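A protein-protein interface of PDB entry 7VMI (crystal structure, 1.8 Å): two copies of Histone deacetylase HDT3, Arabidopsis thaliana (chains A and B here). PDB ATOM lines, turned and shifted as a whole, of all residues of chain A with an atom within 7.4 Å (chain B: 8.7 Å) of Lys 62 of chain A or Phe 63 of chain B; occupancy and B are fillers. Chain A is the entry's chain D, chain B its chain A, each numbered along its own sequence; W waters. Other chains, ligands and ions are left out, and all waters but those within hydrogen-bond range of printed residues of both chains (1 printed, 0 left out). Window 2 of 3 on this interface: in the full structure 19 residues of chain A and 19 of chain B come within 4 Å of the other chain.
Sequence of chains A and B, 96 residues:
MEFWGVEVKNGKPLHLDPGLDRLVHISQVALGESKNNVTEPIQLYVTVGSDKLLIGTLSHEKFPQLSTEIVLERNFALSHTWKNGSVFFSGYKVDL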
ATOM      1  N   THR A  57     -14.727  12.498 -17.616  1.00  0.00           N
ATOM      2  CA  THR A  57     -13.930  13.159 -18.580  1.00  0.00           C
ATOM      3  C   THR A  57     -12.575  12.504 -18.653  1.00  0.00           C
ATOM      4  O   THR A  57     -11.813  12.571 -17.712  1.00  0.00           O
ATOM      5  CB  THR A  57     -13.809  14.638 -18.200  1.00  0.00           C
ATOM      6  OG1 THR A  57     -15.118  15.206 -18.124  1.00  0.00           O
ATOM      7  CG2 THR A  57     -13.038  15.434 -19.308  1.00  0.00           C
ATOM      8  N   LEU A  58     -12.252  11.925 -19.816  1.00  0.00           N
ATOM      9  CA  LEU A  58     -11.039  11.151 -20.033  1.00  0.00           C
ATOM     10  C   LEU A  58      -9.987  11.942 -20.718  1.00  0.00           C
ATOM     11  O   LEU A  58     -10.300  12.906 -21.443  1.00  0.00           O
ATOM     12  CB  LEU A  58     -11.348   9.920 -20.859  1.00  0.00           C
ATOM     13  CG  LEU A  58     -12.448   8.985 -20.282  1.00  0.00           C
ATOM     14  CD1 LEU A  58     -12.562   7.772 -21.210  1.00  0.00           C
ATOM     15  CD2 LEU A  58     -12.174   8.571 -18.863  1.00  0.00           C
ATOM     16  N   SER A  59      -8.725  11.562 -20.506  1.00  0.00           N
ATOM     17  CA  SER A  59      -7.599  12.035 -21.352  1.00  0.00           C
ATOM     18  C   SER A  59      -6.516  10.958 -21.376  1.00  0.00           C
ATOM     19  O   SER A  59      -6.409  10.136 -20.474  1.00  0.00           O
ATOM     20  CB  SER A  59      -7.015  13.318 -20.776  1.00  0.00           C
ATOM     21  OG  SER A  59      -6.463  13.108 -19.461  1.00  0.00           O
ATOM     22  N   HIS A  60      -5.713  10.937 -22.432  1.00  0.00           N
ATOM     23  CA  HIS A  60      -4.593  10.016 -22.572  1.00  0.00           C
ATOM     24  C   HIS A  60      -3.523  10.328 -21.527  1.00  0.00           C
ATOM     25  O   HIS A  60      -2.857   9.461 -21.045  1.00  0.00           O
ATOM     26  CB  HIS A  60      -3.999  10.106 -24.002  1.00  0.00           C
ATOM     27  CG  HIS A  60      -4.969   9.679 -25.050  1.00  0.00           C
ATOM     28  ND1 HIS A  60      -5.741  10.577 -25.771  1.00  0.00           N
ATOM     29  CD2 HIS A  60      -5.349   8.443 -25.453  1.00  0.00           C
ATOM     30  CE1 HIS A  60      -6.558   9.903 -26.572  1.00  0.00           C
ATOM     31  NE2 HIS A  60      -6.318   8.609 -26.415  1.00  0.00           N
ATOM     32  N   GLU A  61      -3.359  11.597 -21.178  1.00  0.00           N
ATOM     33  CA  GLU A  61      -2.340  12.008 -20.247  1.00  0.00           C
ATOM     34  C   GLU A  61      -2.620  11.591 -18.797  1.00  0.00           C
ATOM     35  O   GLU A  61      -1.726  11.233 -18.080  1.00  0.00           O
ATOM     36  CB  GLU A  61      -2.170  13.528 -20.282  1.00  0.00           C
ATOM     37  CG  GLU A  61      -1.653  14.009 -21.617  1.00  0.00           C
ATOM     38  CD  GLU A  61      -2.724  14.156 -22.704  1.00  0.00           C
ATOM     39  OE1 GLU A  61      -3.956  14.170 -22.402  1.00  0.00           O
ATOM     40  OE2 GLU A  61      -2.284  14.297 -23.888  1.00  0.00           O
ATOM     41  N   LYS A  62      -3.864  11.753 -18.364  1.00  0.00           N
ATOM     42  CA  LYS A  62      -4.176  11.715 -16.951  1.00  0.00           C
ATOM     43  C   LYS A  62      -5.275  10.752 -16.612  1.00  0.00           C
ATOM     44  O   LYS A  62      -5.245  10.198 -15.561  1.00  0.00           O
ATOM     45  CB  LYS A  62      -4.546  13.086 -16.436  1.00  0.00           C
ATOM     46  CG  LYS A  62      -3.378  14.051 -16.445  1.00  0.00           C
ATOM     47  CD  LYS A  62      -3.662  15.289 -15.610  1.00  0.00           C
ATOM     48  CE  LYS A  62      -4.559  16.292 -16.371  1.00  0.00           C
ATOM     49  NZ  LYS A  62      -4.213  17.756 -16.202  1.00  0.00           N
ATOM     50  N   PHE A  63      -6.275  10.605 -17.482  1.00  0.00           N
ATOM     51  CA  PHE A  63      -7.437   9.792 -17.162  1.00  0.00           C
ATOM     52  C   PHE A  63      -7.818   8.830 -18.284  1.00  0.00           C
ATOM     53  O   PHE A  63      -8.834   8.991 -18.911  1.00  0.00           O
ATOM     54  CB  PHE A  63      -8.620  10.727 -16.806  1.00  0.00           C
ATOM     55  CG  PHE A  63      -8.247  11.834 -15.856  1.00  0.00           C
ATOM     56  CD1 PHE A  63      -7.912  11.541 -14.543  1.00  0.00           C
ATOM     57  CD2 PHE A  63      -8.171  13.158 -16.303  1.00  0.00           C
ATOM     58  CE1 PHE A  63      -7.533  12.549 -13.668  1.00  0.00           C
ATOM     59  CE2 PHE A  63      -7.802  14.175 -15.467  1.00  0.00           C
ATOM     60  CZ  PHE A  63      -7.489  13.873 -14.123  1.00  0.00           C
ATOM     61  N   PRO A  64      -6.994   7.839 -18.643  1.00  0.00           N
ATOM     62  CA  PRO A  64      -7.280   6.997 -19.802  1.00  0.00           C
ATOM     63  C   PRO A  64      -8.281   5.855 -19.594  1.00  0.00           C
ATOM     64  O   PRO A  64      -8.605   5.167 -20.574  1.00  0.00           O
ATOM     65  CB  PRO A  64      -5.903   6.428 -20.194  1.00  0.00           C
ATOM     66  CG  PRO A  64      -4.999   6.621 -19.004  1.00  0.00           C
ATOM     67  CD  PRO A  64      -5.659   7.614 -18.077  1.00  0.00           C
ATOM     68  N   GLN A  65      -8.774   5.669 -18.360  1.00  0.00           N
ATOM     69  CA  GLN A  65      -9.738   4.643 -18.112  1.00  0.00           C
ATOM     70  C   GLN A  65     -10.438   4.908 -16.812  1.00  0.00           C
ATOM     71  O   GLN A  65      -9.934   5.629 -15.962  1.00  0.00           O
ATOM     72  CB  GLN A  65      -9.088   3.253 -18.064  1.00  0.00           C
ATOM     73  CG  GLN A  65      -7.895   3.113 -17.138  1.00  0.00           C
ATOM     74  CD  GLN A  65      -6.575   3.245 -17.874  1.00  0.00           C
ATOM     75  OE1 GLN A  65      -6.510   3.175 -19.120  1.00  0.00           O
ATOM     76  NE2 GLN A  65      -5.489   3.430 -17.111  1.00  0.00           N
ATOM     77  N   VAL B  29      -5.367  -5.942 -11.822  1.00  0.00           N
ATOM     78  CA  VAL B  29      -4.456  -5.964 -12.918  1.00  0.00           C
ATOM     79  C   VAL B  29      -3.205  -5.203 -12.461  1.00  0.00           C
ATOM     80  O   VAL B  29      -3.302  -4.144 -11.827  1.00  0.00           O
ATOM     81  CB  VAL B  29      -5.070  -5.288 -14.133  1.00  0.00           C
ATOM     82  CG1 VAL B  29      -4.089  -5.329 -15.328  1.00  0.00           C
ATOM     83  CG2 VAL B  29      -6.399  -5.947 -14.497  1.00  0.00           C
ATOM     84  N   ALA B  30      -2.028  -5.783 -12.733  1.00  0.00           N
ATOM     85  CA  ALA B  30      -0.758  -5.146 -12.386  1.00  0.00           C
ATOM     86  C   ALA B  30       0.301  -5.328 -13.465  1.00  0.00           C
ATOM     87  O   ALA B  30       0.542  -6.436 -13.959  1.00  0.00           O
ATOM     88  CB  ALA B  30      -0.247  -5.649 -11.064  1.00  0.00           C
ATOM     89  N   LEU B  31       0.988  -4.228 -13.743  1.00  0.00           N
ATOM     90  CA  LEU B  31       2.116  -4.180 -14.657  1.00  0.00           C
ATOM     91  C   LEU B  31       3.378  -4.699 -13.984  1.00  0.00           C
ATOM     92  O   LEU B  31       3.757  -4.221 -12.923  1.00  0.00           O
ATOM     93  CB  LEU B  31       2.308  -2.737 -15.114  1.00  0.00           C
ATOM     94  CG  LEU B  31       3.324  -2.516 -16.232  1.00  0.00           C
ATOM     95  CD1 LEU B  31       2.960  -3.290 -17.475  1.00  0.00           C
ATOM     96  CD2 LEU B  31       3.378  -1.016 -16.551  1.00  0.00           C
ATOM     97  N   GLY B  32       3.996  -5.702 -14.594  1.00  0.00           N
ATOM     98  CA  GLY B  32       5.226  -6.269 -14.096  1.00  0.00           C
ATOM     99  C   GLY B  32       6.431  -5.349 -14.239  1.00  0.00           C
ATOM    100  O   GLY B  32       6.406  -4.296 -14.852  1.00  0.00           O
ATOM    101  N   PRO B  41       3.305   3.189 -23.331  1.00  0.00           N
ATOM    102  CA  PRO B  41       2.030   2.789 -22.744  1.00  0.00           C
ATOM    103  C   PRO B  41       1.614   1.414 -23.289  1.00  0.00           C
ATOM    104  O   PRO B  41       1.866   1.126 -24.422  1.00  0.00           O
ATOM    105  CB  PRO B  41       1.039   3.879 -23.153  1.00  0.00           C
ATOM    106  CG  PRO B  41       1.925   5.042 -23.578  1.00  0.00           C
ATOM    107  CD  PRO B  41       3.186   4.416 -24.126  1.00  0.00           C
ATOM    108  N   ILE B  42       1.042   0.583 -22.430  1.00  0.00           N
ATOM    109  CA  ILE B  42       0.723  -0.791 -22.706  1.00  0.00           C
ATOM    110  C   ILE B  42      -0.776  -0.966 -22.653  1.00  0.00           C
ATOM    111  O   ILE B  42      -1.378  -0.753 -21.610  1.00  0.00           O
ATOM    112  CB  ILE B  42       1.405  -1.639 -21.632  1.00  0.00           C
ATOM    113  CG1 ILE B  42       2.914  -1.513 -21.815  1.00  0.00           C
ATOM    114  CG2 ILE B  42       0.925  -3.089 -21.647  1.00  0.00           C
ATOM    115  CD1 ILE B  42       3.676  -1.605 -20.551  1.00  0.00           C
ATOM    116  N   LEU B  44      -4.254  -3.181 -22.728  1.00  0.00           N
ATOM    117  CA  LEU B  44      -4.755  -4.448 -22.242  1.00  0.00           C
ATOM    118  C   LEU B  44      -6.082  -4.774 -22.896  1.00  0.00           C
ATOM    119  O   LEU B  44      -6.970  -3.921 -22.985  1.00  0.00           O
ATOM    120  CB  LEU B  44      -5.051  -4.392 -20.744  1.00  0.00           C
ATOM    121  CG  LEU B  44      -4.042  -3.691 -19.867  1.00  0.00           C
ATOM    122  CD1 LEU B  44      -4.614  -3.598 -18.495  1.00  0.00           C
ATOM    123  CD2 LEU B  44      -2.714  -4.446 -19.906  1.00  0.00           C
ATOM    124  N   GLY B  56      -7.872  -1.088 -20.636  1.00  0.00           N
ATOM    125  CA  GLY B  56      -7.073  -0.015 -20.071  1.00  0.00           C
ATOM    126  C   GLY B  56      -5.691   0.074 -20.684  1.00  0.00           C
ATOM    127  O   GLY B  56      -5.288  -0.800 -21.460  1.00  0.00           O
ATOM    128  N   THR B  57      -4.989   1.137 -20.314  1.00  0.00           N
ATOM    129  CA  THR B  57      -3.646   1.416 -20.755  1.00  0.00           C
ATOM    130  C   THR B  57      -2.753   1.712 -19.580  1.00  0.00           C
ATOM    131  O   THR B  57      -2.960   2.691 -18.920  1.00  0.00           O
ATOM    132  CB  THR B  57      -3.647   2.613 -21.726  1.00  0.00           C
ATOM    133  OG1 THR B  57      -4.596   2.356 -22.765  1.00  0.00           O
ATOM    134  CG2 THR B  57      -2.259   2.878 -22.307  1.00  0.00           C
ATOM    135  N   LEU B  58      -1.752   0.858 -19.353  1.00  0.00           N
ATOM    136  CA  LEU B  58      -0.894   0.913 -18.182  1.00  0.00           C
ATOM    137  C   LEU B  58       0.422   1.546 -18.523  1.00  0.00           C
ATOM    138  O   LEU B  58       0.870   1.483 -19.615  1.00  0.00           O
ATOM    139  CB  LEU B  58      -0.647  -0.495 -17.649  1.00  0.00           C
ATOM    140  CG  LEU B  58      -1.879  -1.320 -17.310  1.00  0.00           C
ATOM    141  CD1 LEU B  58      -1.410  -2.639 -16.722  1.00  0.00           C
ATOM    142  CD2 LEU B  58      -2.788  -0.606 -16.337  1.00  0.00           C
ATOM    143  N   SER B  59       1.061   2.146 -17.525  1.00  0.00           N
ATOM    144  CA  SER B  59       2.491   2.557 -17.601  1.00  0.00           C
ATOM    145  C   SER B  59       3.110   2.434 -16.223  1.00  0.00           C
ATOM    146  O   SER B  59       2.390   2.518 -15.214  1.00  0.00           O
ATOM    147  CB  SER B  59       2.619   3.976 -18.094  1.00  0.00           C
ATOM    148  OG  SER B  59       1.986   4.852 -17.181  1.00  0.00           O
ATOM    149  N   HIS B  60       4.435   2.193 -16.166  1.00  0.00           N
ATOM    150  CA  HIS B  60       5.139   2.104 -14.870  1.00  0.00           C
ATOM    151  C   HIS B  60       5.092   3.456 -14.136  1.00  0.00           C
ATOM    152  O   HIS B  60       4.996   3.519 -12.935  1.00  0.00           O
ATOM    153  CB  HIS B  60       6.593   1.687 -15.110  1.00  0.00           C
ATOM    154  CG  HIS B  60       6.724   0.291 -15.600  1.00  0.00           C
ATOM    155  ND1 HIS B  60       6.899  -0.009 -16.928  1.00  0.00           N
ATOM    156  CD2 HIS B  60       6.608  -0.899 -14.945  1.00  0.00           C
ATOM    157  CE1 HIS B  60       6.916  -1.323 -17.081  1.00  0.00           C
ATOM    158  NE2 HIS B  60       6.744  -1.889 -15.892  1.00  0.00           N
ATOM    159  N   GLU B  61       5.151   4.541 -14.922  1.00  0.00           N
ATOM    160  CA  GLU B  61       5.197   5.842 -14.344  1.00  0.00           C
ATOM    161  C   GLU B  61       3.893   6.339 -13.738  1.00  0.00           C
ATOM    162  O   GLU B  61       3.901   7.047 -12.790  1.00  0.00           O
ATOM    163  CB  GLU B  61       5.725   6.813 -15.408  1.00  0.00           C
ATOM    164  CG  GLU B  61       7.233   6.599 -15.589  1.00  0.00           C
ATOM    165  CD  GLU B  61       8.025   6.835 -14.271  1.00  0.00           C
ATOM    166  OE1 GLU B  61       7.481   7.367 -13.276  1.00  0.00           O
ATOM    167  OE2 GLU B  61       9.229   6.532 -14.219  1.00  0.00           O
ATOM    168  N   LYS B  62       2.786   6.046 -14.375  1.00  0.00           N
ATOM    169  CA  LYS B  62       1.523   6.709 -14.069  1.00  0.00           C
ATOM    170  C   LYS B  62       0.387   5.787 -13.793  1.00  0.00           C
ATOM    171  O   LYS B  62      -0.414   6.108 -12.989  1.00  0.00           O
ATOM    172  CB  LYS B  62       1.091   7.545 -15.287  1.00  0.00           C
ATOM    173  CG  LYS B  62       1.941   8.686 -15.520  1.00  0.00           C
ATOM    174  CD  LYS B  62       1.636   9.224 -16.932  1.00  0.00           C
ATOM    175  CE  LYS B  62       0.603  10.318 -16.900  1.00  0.00           C
ATOM    176  NZ  LYS B  62       0.913  11.362 -17.965  1.00  0.00           N
ATOM    177  N   PHE B  63       0.327   4.658 -14.498  1.00  0.00           N
ATOM    178  CA  PHE B  63      -0.793   3.730 -14.314  1.00  0.00           C
ATOM    179  C   PHE B  63      -0.311   2.304 -14.146  1.00  0.00           C
ATOM    180  O   PHE B  63      -0.507   1.492 -15.023  1.00  0.00           O
ATOM    181  CB  PHE B  63      -1.744   3.859 -15.535  1.00  0.00           C
ATOM    182  CG  PHE B  63      -2.102   5.266 -15.861  1.00  0.00           C
ATOM    183  CD1 PHE B  63      -2.860   6.032 -14.985  1.00  0.00           C
ATOM    184  CD2 PHE B  63      -1.597   5.862 -17.012  1.00  0.00           C
ATOM    185  CE1 PHE B  63      -3.132   7.372 -15.267  1.00  0.00           C
ATOM    186  CE2 PHE B  63      -1.857   7.196 -17.291  1.00  0.00           C
ATOM    187  CZ  PHE B  63      -2.589   7.949 -16.408  1.00  0.00           C
ATOM    188  N   PRO B  64       0.391   1.945 -13.069  1.00  0.00           N
ATOM    189  CA  PRO B  64       0.971   0.602 -12.971  1.00  0.00           C
ATOM    190  C   PRO B  64       0.011  -0.517 -12.552  1.00  0.00           C
ATOM    191  O   PRO B  64       0.461  -1.687 -12.510  1.00  0.00           O
ATOM    192  CB  PRO B  64       2.119   0.758 -11.948  1.00  0.00           C
ATOM    193  CG  PRO B  64       1.859   2.083 -11.224  1.00  0.00           C
ATOM    194  CD  PRO B  64       0.820   2.854 -12.004  1.00  0.00           C
ATOM    195  N   GLN B  65      -1.248  -0.174 -12.231  1.00  0.00           N
ATOM    196  CA  GLN B  65      -2.200  -1.195 -11.864  1.00  0.00           C
ATOM    197  C   GLN B  65      -3.604  -0.670 -12.003  1.00  0.00           C
ATOM    198  O   GLN B  65      -3.825   0.544 -12.072  1.00  0.00           O
ATOM    199  CB  GLN B  65      -1.974  -1.647 -10.416  1.00  0.00           C
ATOM    200  CG  GLN B  65      -1.890  -0.501  -9.392  1.00  0.00           C
ATOM    201  CD  GLN B  65      -0.439  -0.153  -9.061  1.00  0.00           C
ATOM    202  OE1 GLN B  65       0.509  -0.887  -9.376  1.00  0.00           O
ATOM    203  NE2 GLN B  65      -0.258   0.934  -8.362  1.00  0.00           N
ATOM    204  N   LEU B  66      -4.576  -1.576 -12.022  1.00  0.00           N
ATOM    205  CA  LEU B  66      -5.994  -1.235 -12.070  1.00  0.00           C
ATOM    206  C   LEU B  66      -6.726  -2.129 -11.100  1.00  0.00           C
ATOM    207  O   LEU B  66      -6.363  -3.319 -10.936  1.00  0.00           O
ATOM    208  CB  LEU B  66      -6.583  -1.536 -13.440  1.00  0.00           C
ATOM    209  CG  LEU B  66      -6.016  -0.798 -14.650  1.00  0.00           C
ATOM    210  CD1 LEU B  66      -6.641  -1.242 -15.953  1.00  0.00           C
ATOM    211  CD2 LEU B  66      -6.190   0.703 -14.536  1.00  0.00           C
ATOM    212  N   VAL B  87       2.005  -8.770 -17.601  1.00  0.00           N
ATOM    213  CA  VAL B  87       0.903  -8.194 -16.892  1.00  0.00           C
ATOM    214  C   VAL B  87       0.201  -9.316 -16.120  1.00  0.00           C
ATOM    215  O   VAL B  87      -0.042 -10.406 -16.672  1.00  0.00           O
ATOM    216  CB  VAL B  87      -0.083  -7.487 -17.832  1.00  0.00           C
ATOM    217  CG1 VAL B  87      -1.228  -6.848 -17.073  1.00  0.00           C
ATOM    218  CG2 VAL B  87       0.652  -6.425 -18.637  1.00  0.00           C
HETATM  219  O   HOH W   1      -7.141   3.032 -22.074  1.00  0.00           O
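Glu 61 of chain A touches Phe 63 of chain B (O to CZ, 3.8 Å).
Phe 63 of chain B touches Lys 62 of chain A.
CD of Pro 64 of chain A touches CZ of Phe 63 of chain B (3.5 Å).
OE1 of Gln 65 of chain A touches CA of Gly 56 of chain B, 3.4 Å away.
NE2 of Gln 65 of chain A touches CD2 of Leu 66 of chain B, at 3.8 Å.
Leu 58 of chain A touches none of the printed residues of chain B.
Printed residues of chain B within 4 Å of Glu 61 of chain A: Lys 62 (2.6 Å) and Phe 63 (3.8 Å).
Of chain B, only Phe 63 (3.5 Å) comes within 4 Å of Lys 62 of chain A.
Printed residues of chain A within 4 Å of Gly 56 of chain B: Gln 65 (3.4 Å).
Phe 63 of chain B touches just these residues of chain A: Glu 61, Lys 62 and Pro 64.
The nearest residue of chain A that does not touch Phe 63 of chain B is Gln 65 of chain A (4.1 Å).
The nearest printed residue of chain B that does not touch Pro 64 of chain A is Thr 57 of chain B (4.4 Å).
OE1 of Gln 65 of chain A sits at hydrogen-bond distance from N of Thr 57 of chain B (2.8 Å).
The side-chain amino group (NZ) of Lys 62 of chain B sits at hydrogen-bond distance from the backbone carbonyl oxygen (O) of Glu 61 of chain A (2.6 Å).
O of Val 29 of chain B sits at hydrogen-bond distance from N of Leu 66 of chain B (2.9 Å).
N of Leu 44 of chain B lies within hydrogen-bond range of O of Gly 56 of chain B (2.9 Å).
The backbone NH of Lys 62 of chain B lies within hydrogen-bond range of the side-chain hydroxyl of Ser 59 of chain B, 3.2 Å away.
N of Phe 63 of chain B is in hydrogen-bond range of OG of Ser 59 of chain B (3.2 Å).
N of Lys 62 of chain A lies within hydrogen-bond range of OG of Ser 59 of chain A, at 3.1 Å.
Glu 61 of chain A touches Lys 62 of chain B, but with the chains exchanged Lys 62 of chain A does not touch Glu 61 of chain B (10.1 Å).
Glu 61 of chain A touches Phe 63 of chain B, but with the chains exchanged Phe 63 of chain A does not touch Glu 61 of chain B (11.6 Å).
Pro 64 of chain A touches Phe 63 of chain B, but with the chains exchanged Phe 63 of chain A does not touch Pro 64 of chain B (11.8 Å).
Gln 65 of chain A touches Thr 57 of chain B, but with the chains exchanged Thr 57 of chain A does not touch Gln 65 of chain B (15.5 Å).
9 positions are printed for both chains.
Of the 9 printed residues of chain A, 4 touch a printed residue of chain B.
Printed residues of chain A that touch a printed residue of chain B: Glu 61, Lys 62, Pro 64 and Gln 65.
Among the printed residues, no Asp or Glu carboxylate lies within 4 Å of a Lys or Arg side-chain nitrogen of the other chain.
Water W1 lies within hydrogen-bond range of OG1 of Thr 57 of chain B (2.7 Å), O of Pro 64 of chain A (3.0 Å) and OE1 of Gln 65 of chain A (3.0 Å).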
